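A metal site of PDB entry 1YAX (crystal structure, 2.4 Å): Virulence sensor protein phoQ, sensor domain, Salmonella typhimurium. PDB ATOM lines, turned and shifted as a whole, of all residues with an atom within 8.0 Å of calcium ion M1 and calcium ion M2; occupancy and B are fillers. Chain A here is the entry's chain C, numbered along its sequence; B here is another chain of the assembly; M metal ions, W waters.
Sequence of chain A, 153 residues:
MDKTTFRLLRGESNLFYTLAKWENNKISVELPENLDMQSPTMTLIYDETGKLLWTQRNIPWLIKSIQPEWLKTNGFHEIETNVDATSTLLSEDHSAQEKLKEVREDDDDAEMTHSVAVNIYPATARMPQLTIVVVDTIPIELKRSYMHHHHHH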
ATOM      1  N   GLU A  78       1.920 -13.490  -8.054  1.00  0.00           N
ATOM      2  CA  GLU A  78       0.855 -13.803  -7.108  1.00  0.00           C
ATOM      3  C   GLU A  78      -0.488 -13.313  -7.602  1.00  0.00           C
ATOM      4  O   GLU A  78      -0.585 -12.243  -8.188  1.00  0.00           O
ATOM      5  CB  GLU A  78       1.144 -13.160  -5.748  1.00  0.00           C
ATOM      6  CG  GLU A  78       2.446 -13.614  -5.112  1.00  0.00           C
ATOM      7  CD  GLU A  78       2.746 -12.919  -3.800  1.00  0.00           C
ATOM      8  OE1 GLU A  78       2.166 -11.847  -3.533  1.00  0.00           O
ATOM      9  OE2 GLU A  78       3.589 -13.452  -3.049  1.00  0.00           O
ATOM     10  N   GLU A  80      -4.042 -12.239  -6.040  1.00  0.00           N
ATOM     11  CA  GLU A  80      -4.885 -11.900  -4.892  1.00  0.00           C
ATOM     12  C   GLU A  80      -6.333 -12.249  -5.264  1.00  0.00           C
ATOM     13  O   GLU A  80      -6.830 -11.806  -6.294  1.00  0.00           O
ATOM     14  CB  GLU A  80      -4.746 -10.411  -4.557  1.00  0.00           C
ATOM     15  CG  GLU A  80      -5.361  -9.948  -3.236  1.00  0.00           C
ATOM     16  CD  GLU A  80      -4.735  -8.663  -2.691  1.00  0.00           C
ATOM     17  OE1 GLU A  80      -5.469  -7.686  -2.342  1.00  0.00           O
ATOM     18  OE2 GLU A  80      -3.497  -8.616  -2.592  1.00  0.00           O
ATOM     19  N   THR A  81      -6.987 -13.043  -4.429  1.00  0.00           N
ATOM     20  CA  THR A  81      -8.382 -13.425  -4.635  1.00  0.00           C
ATOM     21  C   THR A  81      -9.116 -13.458  -3.288  1.00  0.00           C
ATOM     22  O   THR A  81      -8.599 -12.922  -2.317  1.00  0.00           O
ATOM     23  CB  THR A  81      -8.474 -14.765  -5.424  1.00  0.00           C
ATOM     24  OG1 THR A  81      -9.783 -14.914  -6.012  1.00  0.00           O
ATOM     25  CG2 THR A  81      -8.329 -15.984  -4.518  1.00  0.00           C
ATOM     26  N   ALA A 110     -12.077 -11.672   3.712  1.00  0.00           N
ATOM     27  CA  ALA A 110     -10.645 -11.955   3.800  1.00  0.00           C
ATOM     28  C   ALA A 110     -10.051 -12.206   2.419  1.00  0.00           C
ATOM     29  O   ALA A 110     -10.647 -12.890   1.585  1.00  0.00           O
ATOM     30  CB  ALA A 110     -10.396 -13.152   4.714  1.00  0.00           C
ATOM     31  N   GLU A 111      -8.866 -11.647   2.180  1.00  0.00           N
ATOM     32  CA  GLU A 111      -8.150 -11.872   0.922  1.00  0.00           C
ATOM     33  C   GLU A 111      -7.142 -13.036   1.013  1.00  0.00           C
ATOM     34  O   GLU A 111      -6.428 -13.179   2.010  1.00  0.00           O
ATOM     35  CB  GLU A 111      -7.481 -10.592   0.423  1.00  0.00           C
ATOM     36  CG  GLU A 111      -6.305 -10.076   1.237  1.00  0.00           C
ATOM     37  CD  GLU A 111      -5.723  -8.785   0.671  1.00  0.00           C
ATOM     38  OE1 GLU A 111      -6.382  -7.725   0.732  1.00  0.00           O
ATOM     39  OE2 GLU A 111      -4.600  -8.837   0.148  1.00  0.00           O
ATOM     40  N   MET A 112      -7.127 -13.854  -0.035  1.00  0.00           N
ATOM     41  CA  MET A 112      -6.219 -14.988  -0.158  1.00  0.00           C
ATOM     42  C   MET A 112      -5.267 -14.763  -1.334  1.00  0.00           C
ATOM     43  O   MET A 112      -5.665 -14.257  -2.375  1.00  0.00           O
ATOM     44  CB  MET A 112      -7.012 -16.265  -0.420  1.00  0.00           C
ATOM     45  CG  MET A 112      -8.070 -16.604   0.636  1.00  0.00           C
ATOM     46  SD  MET A 112      -7.356 -17.303   2.099  1.00  0.00           S
ATOM     47  CE  MET A 112      -7.359 -15.996   3.147  1.00  0.00           C
ATOM     48  N   THR A 113      -4.017 -15.195  -1.183  1.00  0.00           N
ATOM     49  CA  THR A 113      -3.000 -14.987  -2.194  1.00  0.00           C
ATOM     50  C   THR A 113      -2.378 -16.307  -2.631  1.00  0.00           C
ATOM     51  O   THR A 113      -1.917 -17.078  -1.806  1.00  0.00           O
ATOM     52  CB  THR A 113      -1.930 -14.066  -1.618  1.00  0.00           C
ATOM     53  OG1 THR A 113      -2.577 -12.909  -1.059  1.00  0.00           O
ATOM     54  CG2 THR A 113      -1.003 -13.508  -2.724  1.00  0.00           C
ATOM     55  N   GLU A 141      -1.786 -17.216   3.056  1.00  0.00           N
ATOM     56  CA  GLU A 141      -2.407 -16.825   4.313  1.00  0.00           C
ATOM     57  C   GLU A 141      -2.686 -18.004   5.239  1.00  0.00           C
ATOM     58  O   GLU A 141      -2.875 -17.822   6.438  1.00  0.00           O
ATOM     59  CB  GLU A 141      -3.712 -16.069   4.059  1.00  0.00           C
ATOM     60  CG  GLU A 141      -3.518 -14.638   3.569  1.00  0.00           C
ATOM     61  CD  GLU A 141      -3.243 -14.533   2.063  1.00  0.00           C
ATOM     62  OE1 GLU A 141      -3.207 -13.384   1.553  1.00  0.00           O
ATOM     63  OE2 GLU A 141      -3.038 -15.591   1.409  1.00  0.00           O
ATOM     64  N   GLU B  78      -0.059  -0.170  -5.655  1.00  0.00           N
ATOM     65  CA  GLU B  78      -0.365  -0.267  -4.238  1.00  0.00           C
ATOM     66  C   GLU B  78       0.746  -1.026  -3.538  1.00  0.00           C
ATOM     67  O   GLU B  78       1.334  -1.940  -4.107  1.00  0.00           O
ATOM     68  CB  GLU B  78      -1.713  -0.956  -4.015  1.00  0.00           C
ATOM     69  CG  GLU B  78      -2.850  -0.003  -3.639  1.00  0.00           C
ATOM     70  CD  GLU B  78      -4.139  -0.259  -4.384  1.00  0.00           C
ATOM     71  OE1 GLU B  78      -4.913  -1.166  -3.998  1.00  0.00           O
ATOM     72  OE2 GLU B  78      -4.393   0.466  -5.371  1.00  0.00           O
ATOM     73  N   GLU B  80       1.439  -2.938   0.129  1.00  0.00           N
ATOM     74  CA  GLU B  80       0.871  -3.432   1.377  1.00  0.00           C
ATOM     75  C   GLU B  80       1.972  -3.510   2.461  1.00  0.00           C
ATOM     76  O   GLU B  80       3.076  -4.059   2.239  1.00  0.00           O
ATOM     77  CB  GLU B  80       0.165  -4.808   1.169  1.00  0.00           C
ATOM     78  CG  GLU B  80      -1.324  -4.691   0.808  1.00  0.00           C
ATOM     79  CD  GLU B  80      -2.076  -6.021   0.598  1.00  0.00           C
ATOM     80  OE1 GLU B  80      -3.095  -5.979  -0.139  1.00  0.00           O
ATOM     81  OE2 GLU B  80      -1.691  -7.082   1.147  1.00  0.00           O
ATOM     82  N   THR B  81       1.666  -2.994   3.649  1.00  0.00           N
ATOM     83  CA  THR B  81       2.432  -3.305   4.869  1.00  0.00           C
ATOM     84  C   THR B  81       1.450  -3.383   6.077  1.00  0.00           C
ATOM     85  O   THR B  81       0.179  -3.409   5.894  1.00  0.00           O
ATOM     86  CB  THR B  81       3.521  -2.235   5.096  1.00  0.00           C
ATOM     87  OG1 THR B  81       4.264  -2.593   6.297  1.00  0.00           O
ATOM     88  CG2 THR B  81       2.880  -0.845   5.374  1.00  0.00           C
ATOM     89  N   GLU B 111      -3.618  -5.140   8.143  1.00  0.00           N
ATOM     90  CA  GLU B 111      -2.983  -4.859   6.838  1.00  0.00           C
ATOM     91  C   GLU B 111      -3.291  -3.445   6.267  1.00  0.00           C
ATOM     92  O   GLU B 111      -4.419  -3.175   5.846  1.00  0.00           O
ATOM     93  CB  GLU B 111      -3.397  -5.919   5.818  1.00  0.00           C
ATOM     94  CG  GLU B 111      -2.679  -5.813   4.461  1.00  0.00           C
ATOM     95  CD  GLU B 111      -2.436  -7.160   3.798  1.00  0.00           C
ATOM     96  OE1 GLU B 111      -1.243  -7.459   3.365  1.00  0.00           O
ATOM     97  OE2 GLU B 111      -3.429  -7.933   3.763  1.00  0.00           O
ATOM     98  N   MET B 112      -2.280  -2.576   6.243  1.00  0.00           N
ATOM     99  CA  MET B 112      -2.379  -1.272   5.532  1.00  0.00           C
ATOM    100  C   MET B 112      -1.898  -1.393   4.076  1.00  0.00           C
ATOM    101  O   MET B 112      -0.934  -2.089   3.792  1.00  0.00           O
ATOM    102  CB  MET B 112      -1.526  -0.174   6.219  1.00  0.00           C
ATOM    103  CG  MET B 112      -1.869   0.132   7.718  1.00  0.00           C
ATOM    104  SD  MET B 112      -3.419   1.046   7.910  1.00  0.00           S
ATOM    105  CE  MET B 112      -4.540  -0.522   8.368  1.00  0.00           C
ATOM    106  N   THR B 113      -2.577  -0.712   3.161  1.00  0.00           N
ATOM    107  CA  THR B 113      -2.072  -0.585   1.796  1.00  0.00           C
ATOM    108  C   THR B 113      -1.968   0.891   1.408  1.00  0.00           C
ATOM    109  O   THR B 113      -2.793   1.701   1.829  1.00  0.00           O
ATOM    110  CB  THR B 113      -2.912  -1.394   0.773  1.00  0.00           C
ATOM    111  OG1 THR B 113      -2.540  -1.006  -0.561  1.00  0.00           O
ATOM    112  CG2 THR B 113      -4.382  -1.028   0.844  1.00  0.00           C
ATOM    113  N   ILE B 140      -5.080   3.679   2.296  1.00  0.00           N
ATOM    114  CA  ILE B 140      -6.450   3.790   1.782  1.00  0.00           C
ATOM    115  C   ILE B 140      -7.501   3.333   2.809  1.00  0.00           C
ATOM    116  O   ILE B 140      -8.692   3.610   2.630  1.00  0.00           O
ATOM    117  CB  ILE B 140      -6.631   3.017   0.425  1.00  0.00           C
ATOM    118  CG1 ILE B 140      -6.741   1.503   0.639  1.00  0.00           C
ATOM    119  CG2 ILE B 140      -5.476   3.337  -0.549  1.00  0.00           C
ATOM    120  CD1 ILE B 140      -8.182   0.981   0.828  1.00  0.00           C
ATOM    121  N   GLU B 141      -7.073   2.644   3.865  1.00  0.00           N
ATOM    122  CA  GLU B 141      -7.970   2.163   4.923  1.00  0.00           C
ATOM    123  C   GLU B 141      -8.577   3.299   5.774  1.00  0.00           C
ATOM    124  O   GLU B 141      -9.660   3.136   6.330  1.00  0.00           O
ATOM    125  CB  GLU B 141      -7.261   1.149   5.840  1.00  0.00           C
ATOM    126  CG  GLU B 141      -7.278  -0.299   5.334  1.00  0.00           C
ATOM    127  CD  GLU B 141      -6.289  -0.584   4.194  1.00  0.00           C
ATOM    128  OE1 GLU B 141      -6.547  -1.527   3.426  1.00  0.00           O
ATOM    129  OE2 GLU B 141      -5.270   0.114   4.068  1.00  0.00           O
HETATM  130 CA    CA M   1      -5.400  -6.072  -0.606  1.00  0.00          CA
HETATM  131 CA    CA M   2      -2.920  -9.015   1.705  1.00  0.00          CA
HETATM  132  O   HOH W   1      -3.584  -4.850  -2.362  1.00  0.00           O
HETATM  133  O   HOH W   2      -2.681 -10.168  -0.265  1.00  0.00           O
HETATM  134  O   HOH W   3      -5.332  -5.770   1.611  1.00  0.00           O
HETATM  135  O   HOH W   4      -3.634 -11.161   2.792  1.00  0.00           O
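Water W2 binds calcium ion M2 (2.3 Å).
Calcium ion M2 is bound by the side-chain carboxylate (OE2) of Glu 111 of chain A, 2.3 Å away.
OE2 of Glu 80 of chain B binds calcium ion M2 (2.4 Å).
OE2 of Glu 111 of chain B is bound to calcium ion M2 (2.4 Å).
Water W4 binds calcium ion M2 (2.5 Å).
Calcium ion M2 is bound by OE1 of Glu 111 of chain B.
Calcium ion M2 has six donor atoms within binding distance.
The nearest printed residue that does not touch calcium ion M1 is Glu 111 of chain B (5.1 Å).
Calcium ion M1 is bound by water W3 (2.2 Å).
OE1 of Glu 111 of chain A is bound to calcium ion M1 (2.3 Å).
Calcium ion M1 is bound by the side-chain carboxylate (OE1) of Glu 80 of chain B, at 2.4 Å.
OE1 of Glu 80 of chain A is bound to calcium ion M1, 2.4 Å away.
Water W1 is bound to calcium ion M1 (2.8 Å).
Slightly farther from calcium ion M1 lies OE2 of Glu 111 of chain A (3.0 Å).
Water W2 bridges the side-chain hydroxyl of Thr 113 of chain A (2.9 Å) and the side-chain carboxylate of Glu 80 of chain A (2.9 Å).
Within 4 Å of calcium ion M2: Glu 111 of chain A, Glu 80 of chain B and Glu 111 of chain B.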
